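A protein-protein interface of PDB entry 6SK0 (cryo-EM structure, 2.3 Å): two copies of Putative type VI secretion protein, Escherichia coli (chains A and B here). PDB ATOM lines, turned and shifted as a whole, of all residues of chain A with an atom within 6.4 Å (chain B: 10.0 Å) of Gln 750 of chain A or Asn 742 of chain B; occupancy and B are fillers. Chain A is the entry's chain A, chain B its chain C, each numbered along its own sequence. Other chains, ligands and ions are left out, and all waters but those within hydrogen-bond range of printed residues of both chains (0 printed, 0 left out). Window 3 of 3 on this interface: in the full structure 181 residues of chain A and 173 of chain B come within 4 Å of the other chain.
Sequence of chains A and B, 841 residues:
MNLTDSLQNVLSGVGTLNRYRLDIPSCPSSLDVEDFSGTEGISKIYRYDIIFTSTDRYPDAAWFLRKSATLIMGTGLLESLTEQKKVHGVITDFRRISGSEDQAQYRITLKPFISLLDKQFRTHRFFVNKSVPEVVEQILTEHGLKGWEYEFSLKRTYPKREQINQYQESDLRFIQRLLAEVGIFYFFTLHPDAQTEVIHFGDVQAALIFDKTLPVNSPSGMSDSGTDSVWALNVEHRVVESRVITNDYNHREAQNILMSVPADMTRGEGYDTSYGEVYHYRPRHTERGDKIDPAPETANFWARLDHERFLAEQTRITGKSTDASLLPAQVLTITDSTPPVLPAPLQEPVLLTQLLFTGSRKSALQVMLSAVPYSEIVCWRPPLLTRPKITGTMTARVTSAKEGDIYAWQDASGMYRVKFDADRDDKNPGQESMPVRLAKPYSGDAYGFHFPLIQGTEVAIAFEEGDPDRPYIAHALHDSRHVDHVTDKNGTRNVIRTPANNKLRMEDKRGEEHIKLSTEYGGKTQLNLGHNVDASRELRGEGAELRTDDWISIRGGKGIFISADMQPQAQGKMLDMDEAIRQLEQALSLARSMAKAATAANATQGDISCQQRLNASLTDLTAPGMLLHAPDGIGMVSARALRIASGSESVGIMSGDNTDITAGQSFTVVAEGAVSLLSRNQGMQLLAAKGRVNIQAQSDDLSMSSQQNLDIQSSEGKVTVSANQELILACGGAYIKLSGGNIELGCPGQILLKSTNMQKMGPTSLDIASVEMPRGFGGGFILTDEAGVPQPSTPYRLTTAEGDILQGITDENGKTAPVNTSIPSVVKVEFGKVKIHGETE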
ATOM      1  N   CYS A 731      16.833 -10.276  16.159  1.00  0.00           N
ATOM      2  CA  CYS A 731      17.583  -9.486  17.124  1.00  0.00           C
ATOM      3  C   CYS A 731      17.396  -8.020  16.785  1.00  0.00           C
ATOM      4  O   CYS A 731      17.694  -7.608  15.662  1.00  0.00           O
ATOM      5  CB  CYS A 731      19.060  -9.845  17.118  1.00  0.00           C
ATOM      6  SG  CYS A 731      20.024  -8.820  18.226  1.00  0.00           S
ATOM      7  N   GLY A 732      16.909  -7.245  17.746  1.00  0.00           N
ATOM      8  CA  GLY A 732      16.870  -5.799  17.608  1.00  0.00           C
ATOM      9  C   GLY A 732      16.078  -5.291  16.425  1.00  0.00           C
ATOM     10  O   GLY A 732      16.509  -4.346  15.758  1.00  0.00           O
ATOM     11  N   ALA A 734      15.774  -6.540  13.555  1.00  0.00           N
ATOM     12  CA  ALA A 734      16.191  -7.330  12.413  1.00  0.00           C
ATOM     13  C   ALA A 734      15.733  -8.772  12.572  1.00  0.00           C
ATOM     14  O   ALA A 734      15.634  -9.298  13.681  1.00  0.00           O
ATOM     15  CB  ALA A 734      17.707  -7.277  12.253  1.00  0.00           C
ATOM     16  N   CYS A 747      14.889  -5.825   8.270  1.00  0.00           N
ATOM     17  CA  CYS A 747      15.501  -5.032   9.319  1.00  0.00           C
ATOM     18  C   CYS A 747      15.130  -3.576   9.111  1.00  0.00           C
ATOM     19  O   CYS A 747      14.930  -3.146   7.971  1.00  0.00           O
ATOM     20  CB  CYS A 747      17.025  -5.204   9.343  1.00  0.00           C
ATOM     21  SG  CYS A 747      17.918  -4.463   7.994  1.00  0.00           S
ATOM     22  N   PRO A 748      15.000  -2.803  10.188  1.00  0.00           N
ATOM     23  CA  PRO A 748      14.760  -1.365  10.027  1.00  0.00           C
ATOM     24  C   PRO A 748      15.987  -0.606   9.577  1.00  0.00           C
ATOM     25  O   PRO A 748      15.849   0.497   9.040  1.00  0.00           O
ATOM     26  CB  PRO A 748      14.323  -0.932  11.427  1.00  0.00           C
ATOM     27  CG  PRO A 748      15.018  -1.889  12.322  1.00  0.00           C
ATOM     28  CD  PRO A 748      15.052  -3.199  11.604  1.00  0.00           C
ATOM     29  N   GLY A 749      17.178  -1.154   9.781  1.00  0.00           N
ATOM     30  CA  GLY A 749      18.393  -0.510   9.348  1.00  0.00           C
ATOM     31  C   GLY A 749      18.813  -0.972   7.975  1.00  0.00           C
ATOM     32  O   GLY A 749      18.004  -0.996   7.049  1.00  0.00           O
ATOM     33  N   GLN A 750      20.067  -1.366   7.827  1.00  0.00           N
ATOM     34  CA  GLN A 750      20.596  -1.737   6.531  1.00  0.00           C
ATOM     35  C   GLN A 750      21.008  -3.200   6.512  1.00  0.00           C
ATOM     36  O   GLN A 750      21.404  -3.761   7.535  1.00  0.00           O
ATOM     37  CB  GLN A 750      21.775  -0.850   6.156  1.00  0.00           C
ATOM     38  CG  GLN A 750      22.999  -1.046   6.999  1.00  0.00           C
ATOM     39  CD  GLN A 750      24.217  -0.412   6.374  1.00  0.00           C
ATOM     40  OE1 GLN A 750      24.134   0.661   5.777  1.00  0.00           O
ATOM     41  NE2 GLN A 750      25.359  -1.076   6.494  1.00  0.00           N
ATOM     42  N   ILE A 751      20.893  -3.808   5.343  1.00  0.00           N
ATOM     43  CA  ILE A 751      21.434  -5.134   5.095  1.00  0.00           C
ATOM     44  C   ILE A 751      22.763  -4.962   4.384  1.00  0.00           C
ATOM     45  O   ILE A 751      22.822  -4.424   3.274  1.00  0.00           O
ATOM     46  CB  ILE A 751      20.464  -5.984   4.266  1.00  0.00           C
ATOM     47  CG1 ILE A 751      19.143  -6.134   5.010  1.00  0.00           C
ATOM     48  CG2 ILE A 751      21.077  -7.325   3.958  1.00  0.00           C
ATOM     49  CD1 ILE A 751      18.097  -6.873   4.251  1.00  0.00           C
ATOM     50  N   LEU A 752      23.834  -5.401   5.025  1.00  0.00           N
ATOM     51  CA  LEU A 752      25.182  -5.229   4.513  1.00  0.00           C
ATOM     52  C   LEU A 752      25.744  -6.586   4.125  1.00  0.00           C
ATOM     53  O   LEU A 752      25.753  -7.513   4.937  1.00  0.00           O
ATOM     54  CB  LEU A 752      26.067  -4.546   5.550  1.00  0.00           C
ATOM     55  CG  LEU A 752      27.525  -4.303   5.182  1.00  0.00           C
ATOM     56  CD1 LEU A 752      27.655  -3.553   3.863  1.00  0.00           C
ATOM     57  CD2 LEU A 752      28.204  -3.540   6.297  1.00  0.00           C
ATOM     58  N   GLN B 725      20.881  -8.443  22.179  1.00  0.00           N
ATOM     59  CA  GLN B 725      21.943  -7.545  21.764  1.00  0.00           C
ATOM     60  C   GLN B 725      22.468  -7.848  20.377  1.00  0.00           C
ATOM     61  O   GLN B 725      22.672  -6.930  19.583  1.00  0.00           O
ATOM     62  CB  GLN B 725      23.100  -7.612  22.756  1.00  0.00           C
ATOM     63  CG  GLN B 725      22.759  -7.080  24.118  1.00  0.00           C
ATOM     64  CD  GLN B 725      23.941  -7.107  25.046  1.00  0.00           C
ATOM     65  OE1 GLN B 725      24.163  -6.176  25.812  1.00  0.00           O
ATOM     66  NE2 GLN B 725      24.714  -8.180  24.984  1.00  0.00           N
ATOM     67  N   GLU B 726      22.688  -9.116  20.066  1.00  0.00           N
ATOM     68  CA  GLU B 726      23.416  -9.465  18.860  1.00  0.00           C
ATOM     69  C   GLU B 726      23.236 -10.949  18.601  1.00  0.00           C
ATOM     70  O   GLU B 726      23.501 -11.769  19.480  1.00  0.00           O
ATOM     71  CB  GLU B 726      24.894  -9.100  19.025  1.00  0.00           C
ATOM     72  CG  GLU B 726      25.803  -9.459  17.890  1.00  0.00           C
ATOM     73  CD  GLU B 726      27.158  -8.775  18.007  1.00  0.00           C
ATOM     74  OE1 GLU B 726      27.937  -9.129  18.921  1.00  0.00           O
ATOM     75  OE2 GLU B 726      27.453  -7.876  17.194  1.00  0.00           O
ATOM     76  N   LEU B 727      22.782 -11.287  17.410  1.00  0.00           N
ATOM     77  CA  LEU B 727      22.683 -12.667  16.973  1.00  0.00           C
ATOM     78  C   LEU B 727      23.745 -12.900  15.912  1.00  0.00           C
ATOM     79  O   LEU B 727      23.738 -12.245  14.868  1.00  0.00           O
ATOM     80  CB  LEU B 727      21.288 -12.973  16.441  1.00  0.00           C
ATOM     81  CG  LEU B 727      20.874 -14.442  16.378  1.00  0.00           C
ATOM     82  CD1 LEU B 727      19.365 -14.568  16.405  1.00  0.00           C
ATOM     83  CD2 LEU B 727      21.423 -15.105  15.150  1.00  0.00           C
ATOM     84  N   ILE B 728      24.650 -13.832  16.174  1.00  0.00           N
ATOM     85  CA  ILE B 728      25.761 -14.120  15.282  1.00  0.00           C
ATOM     86  C   ILE B 728      25.736 -15.592  14.910  1.00  0.00           C
ATOM     87  O   ILE B 728      25.720 -16.461  15.786  1.00  0.00           O
ATOM     88  CB  ILE B 728      27.112 -13.753  15.918  1.00  0.00           C
ATOM     89  CG1 ILE B 728      27.148 -12.270  16.260  1.00  0.00           C
ATOM     90  CG2 ILE B 728      28.244 -14.113  14.989  1.00  0.00           C
ATOM     91  CD1 ILE B 728      28.429 -11.829  16.891  1.00  0.00           C
ATOM     92  N   TYR B 735      30.038 -15.119   8.337  1.00  0.00           N
ATOM     93  CA  TYR B 735      29.170 -14.854   9.466  1.00  0.00           C
ATOM     94  C   TYR B 735      27.921 -14.124   9.007  1.00  0.00           C
ATOM     95  O   TYR B 735      27.917 -13.426   7.993  1.00  0.00           O
ATOM     96  CB  TYR B 735      29.877 -14.048  10.557  1.00  0.00           C
ATOM     97  CG  TYR B 735      30.195 -12.644  10.143  1.00  0.00           C
ATOM     98  CD1 TYR B 735      31.387 -12.350   9.513  1.00  0.00           C
ATOM     99  CD2 TYR B 735      29.297 -11.614  10.366  1.00  0.00           C
ATOM    100  CE1 TYR B 735      31.682 -11.073   9.124  1.00  0.00           C
ATOM    101  CE2 TYR B 735      29.584 -10.334   9.977  1.00  0.00           C
ATOM    102  CZ  TYR B 735      30.779 -10.069   9.356  1.00  0.00           C
ATOM    103  OH  TYR B 735      31.073  -8.793   8.965  1.00  0.00           O
ATOM    104  N   ILE B 736      26.861 -14.299   9.779  1.00  0.00           N
ATOM    105  CA  ILE B 736      25.657 -13.495   9.682  1.00  0.00           C
ATOM    106  C   ILE B 736      25.430 -12.881  11.048  1.00  0.00           C
ATOM    107  O   ILE B 736      25.335 -13.600  12.048  1.00  0.00           O
ATOM    108  CB  ILE B 736      24.445 -14.321   9.241  1.00  0.00           C
ATOM    109  CG1 ILE B 736      24.689 -14.907   7.855  1.00  0.00           C
ATOM    110  CG2 ILE B 736      23.206 -13.469   9.257  1.00  0.00           C
ATOM    111  CD1 ILE B 736      23.593 -15.777   7.374  1.00  0.00           C
ATOM    112  N   LYS B 737      25.367 -11.561  11.099  1.00  0.00           N
ATOM    113  CA  LYS B 737      25.176 -10.849  12.346  1.00  0.00           C
ATOM    114  C   LYS B 737      23.910 -10.016  12.275  1.00  0.00           C
ATOM    115  O   LYS B 737      23.722  -9.235  11.338  1.00  0.00           O
ATOM    116  CB  LYS B 737      26.376  -9.971  12.673  1.00  0.00           C
ATOM    117  CG  LYS B 737      26.217  -9.214  13.962  1.00  0.00           C
ATOM    118  CD  LYS B 737      27.310  -8.196  14.134  1.00  0.00           C
ATOM    119  CE  LYS B 737      28.671  -8.822  13.954  1.00  0.00           C
ATOM    120  NZ  LYS B 737      29.723  -7.792  13.752  1.00  0.00           N
ATOM    121  N   LEU B 738      23.044 -10.203  13.250  1.00  0.00           N
ATOM    122  CA  LEU B 738      21.878  -9.363  13.468  1.00  0.00           C
ATOM    123  C   LEU B 738      22.163  -8.552  14.720  1.00  0.00           C
ATOM    124  O   LEU B 738      22.241  -9.111  15.818  1.00  0.00           O
ATOM    125  CB  LEU B 738      20.615 -10.200  13.630  1.00  0.00           C
ATOM    126  CG  LEU B 738      19.915 -10.756  12.399  1.00  0.00           C
ATOM    127  CD1 LEU B 738      20.752 -11.811  11.736  1.00  0.00           C
ATOM    128  CD2 LEU B 738      18.556 -11.322  12.782  1.00  0.00           C
ATOM    129  N   SER B 739      22.358  -7.251  14.555  1.00  0.00           N
ATOM    130  CA  SER B 739      22.659  -6.378  15.679  1.00  0.00           C
ATOM    131  C   SER B 739      22.308  -4.953  15.292  1.00  0.00           C
ATOM    132  O   SER B 739      22.281  -4.601  14.112  1.00  0.00           O
ATOM    133  CB  SER B 739      24.126  -6.473  16.104  1.00  0.00           C
ATOM    134  OG  SER B 739      24.981  -6.012  15.084  1.00  0.00           O
ATOM    135  N   GLY B 740      22.079  -4.137  16.303  1.00  0.00           N
ATOM    136  CA  GLY B 740      21.488  -2.840  16.059  1.00  0.00           C
ATOM    137  C   GLY B 740      20.131  -3.093  15.456  1.00  0.00           C
ATOM    138  O   GLY B 740      19.310  -3.832  16.007  1.00  0.00           O
ATOM    139  N   GLY B 741      19.886  -2.516  14.297  1.00  0.00           N
ATOM    140  CA  GLY B 741      18.728  -2.904  13.530  1.00  0.00           C
ATOM    141  C   GLY B 741      19.184  -3.353  12.167  1.00  0.00           C
ATOM    142  O   GLY B 741      18.470  -3.202  11.177  1.00  0.00           O
ATOM    143  N   ASN B 742      20.389  -3.894  12.108  1.00  0.00           N
ATOM    144  CA  ASN B 742      21.037  -4.219  10.856  1.00  0.00           C
ATOM    145  C   ASN B 742      21.223  -5.718  10.718  1.00  0.00           C
ATOM    146  O   ASN B 742      21.213  -6.468  11.695  1.00  0.00           O
ATOM    147  CB  ASN B 742      22.394  -3.528  10.744  1.00  0.00           C
ATOM    148  CG  ASN B 742      22.291  -2.038  10.879  1.00  0.00           C
ATOM    149  OD1 ASN B 742      21.434  -1.410  10.270  1.00  0.00           O
ATOM    150  ND2 ASN B 742      23.158  -1.459  11.688  1.00  0.00           N
ATOM    151  N   ILE B 743      21.394  -6.139   9.476  1.00  0.00           N
ATOM    152  CA  ILE B 743      21.805  -7.490   9.143  1.00  0.00           C
ATOM    153  C   ILE B 743      23.098  -7.387   8.359  1.00  0.00           C
ATOM    154  O   ILE B 743      23.173  -6.654   7.370  1.00  0.00           O
ATOM    155  CB  ILE B 743      20.732  -8.235   8.334  1.00  0.00           C
ATOM    156  CG1 ILE B 743      19.399  -8.207   9.069  1.00  0.00           C
ATOM    157  CG2 ILE B 743      21.178  -9.646   8.058  1.00  0.00           C
ATOM    158  CD1 ILE B 743      18.283  -8.871   8.324  1.00  0.00           C
ATOM    159  N   GLU B 744      24.110  -8.114   8.803  1.00  0.00           N
ATOM    160  CA  GLU B 744      25.408  -8.124   8.153  1.00  0.00           C
ATOM    161  C   GLU B 744      25.750  -9.551   7.763  1.00  0.00           C
ATOM    162  O   GLU B 744      25.786 -10.441   8.617  1.00  0.00           O
ATOM    163  CB  GLU B 744      26.471  -7.532   9.071  1.00  0.00           C
ATOM    164  CG  GLU B 744      27.828  -7.399   8.445  1.00  0.00           C
ATOM    165  CD  GLU B 744      28.784  -6.629   9.329  1.00  0.00           C
ATOM    166  OE1 GLU B 744      28.319  -5.758  10.092  1.00  0.00           O
ATOM    167  OE2 GLU B 744      29.999  -6.895   9.272  1.00  0.00           O
ATOM    168  N   LEU B 745      25.975  -9.767   6.481  1.00  0.00           N
ATOM    169  CA  LEU B 745      26.450 -11.037   5.951  1.00  0.00           C
ATOM    170  C   LEU B 745      27.875 -10.803   5.485  1.00  0.00           C
ATOM    171  O   LEU B 745      28.104 -10.147   4.467  1.00  0.00           O
ATOM    172  CB  LEU B 745      25.572 -11.533   4.815  1.00  0.00           C
ATOM    173  CG  LEU B 745      24.236 -12.159   5.170  1.00  0.00           C
ATOM    174  CD1 LEU B 745      23.219 -11.083   5.424  1.00  0.00           C
ATOM    175  CD2 LEU B 745      23.789 -13.043   4.041  1.00  0.00           C
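Gln 750 of chain A touches just these residues of chain B: Asn 742 and Ile 743.
Printed residues of chain A within 4 Å of Asn 742 of chain B: Ala 734 (3.6 Å), Gly 749 (3.3 Å) and Gln 750 (2.8 Å).
Printed residues of chain B within 4 Å of Gly 749 of chain A: Gly 741 and Asn 742.
Of the printed residues of chain B, Ile 751 of chain A touches Ile 743.
Of the printed residues of chain A, Glu 726 of chain B touches Cys 731.
Of the printed residues of chain B, Leu 752 of chain A touches Ile 743, Glu 744 and Leu 745.
Of the printed residues of chain A, Ile 743 of chain B touches Ala 734, Cys 747, Gln 750, Ile 751 and Leu 752.
The nearest residue of chain B that does not touch Gln 750 of chain A is Gly 741 of chain B (4.1 Å).
The nearest residue of chain A that does not touch Asn 742 of chain B is Cys 747 of chain A (4.2 Å).
Among the printed residues, merely in contact across the chains: Ile 751 of chain A with Ile 743 of chain B, Leu 752 of chain A with Glu 744 of chain B, Gly 749 of chain A with Asn 742 of chain B, Pro 748 of chain A with Gly 741 of chain B, Gly 732 of chain A with Gly 741 of chain B, Ala 734 of chain A with Asn 742 of chain B, Ala 734 of chain A with Leu 738 of chain B, Ala 734 of chain A with Ile 743 of chain B and Cys 747 of chain A with Ile 743 of chain B.
Of the 9 printed residues of chain A, 9 touch a printed residue of chain B.
Hydrophobic or aromatic side chains of chain A that line the printed part of chain B: Ala 734 and Pro 748.
Among the printed residues, 20 pairs touch across the chains.
The side-chain sulfur of Cys 731 of chain A lies close to the backbone carbonyl oxygen of Gln 725 of chain B, at 3.5 Å.
N of Glu 726 of chain B sits at hydrogen-bond distance from SG of Cys 731 of chain A (3.3 Å).
The side-chain sulfur of Cys 731 of chain A is in hydrogen-bond range of the backbone NH of Leu 727 of chain B (3.8 Å).
O of Leu 738 of chain B sits at hydrogen-bond distance from SG of Cys 731 of chain A.
The side-chain sulfur (SG) of Cys 747 of chain A sits close to the backbone carbonyl oxygen (O) of Gly 741 of chain B (3.5 Å).
N of Gly 749 of chain A lies within hydrogen-bond range of O of Gly 741 of chain B (2.8 Å).
The backbone NH of Gln 750 of chain A sits at hydrogen-bond distance from the side-chain amide oxygen of Asn 742 of chain B, at 2.8 Å.
The backbone NH (N) of Ile 743 of chain B sits at hydrogen-bond distance from the backbone carbonyl oxygen (O) of Gln 750 of chain A (3.1 Å).
O of Ile 743 of chain B sits at hydrogen-bond distance from N of Leu 752 of chain A (2.7 Å).
N of Leu 745 of chain B lies within hydrogen-bond range of O of Leu 752 of chain A.
The backbone carbonyl oxygen (O) of Gly 740 of chain B lies close to the backbone carbonyl oxygen (O) of Gly 732 of chain A, 2.9 Å away.
No position is printed for both chains.
The side-chain sulfur of Cys 747 of chain A lies within hydrogen-bond range of the backbone carbonyl oxygen of Gly 749 of chain A (3.6 Å).
The side-chain sulfur of Cys 747 of chain A is in hydrogen-bond range of the backbone carbonyl oxygen of Gln 750 of chain A, 3.6 Å away.
The backbone carbonyl oxygen of Leu 727 of chain B is in hydrogen-bond range of the backbone NH of Leu 738 of chain B, at 2.7 Å.
O of Glu 744 of chain B is in hydrogen-bond range of N of Lys 737 of chain B (2.8 Å).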
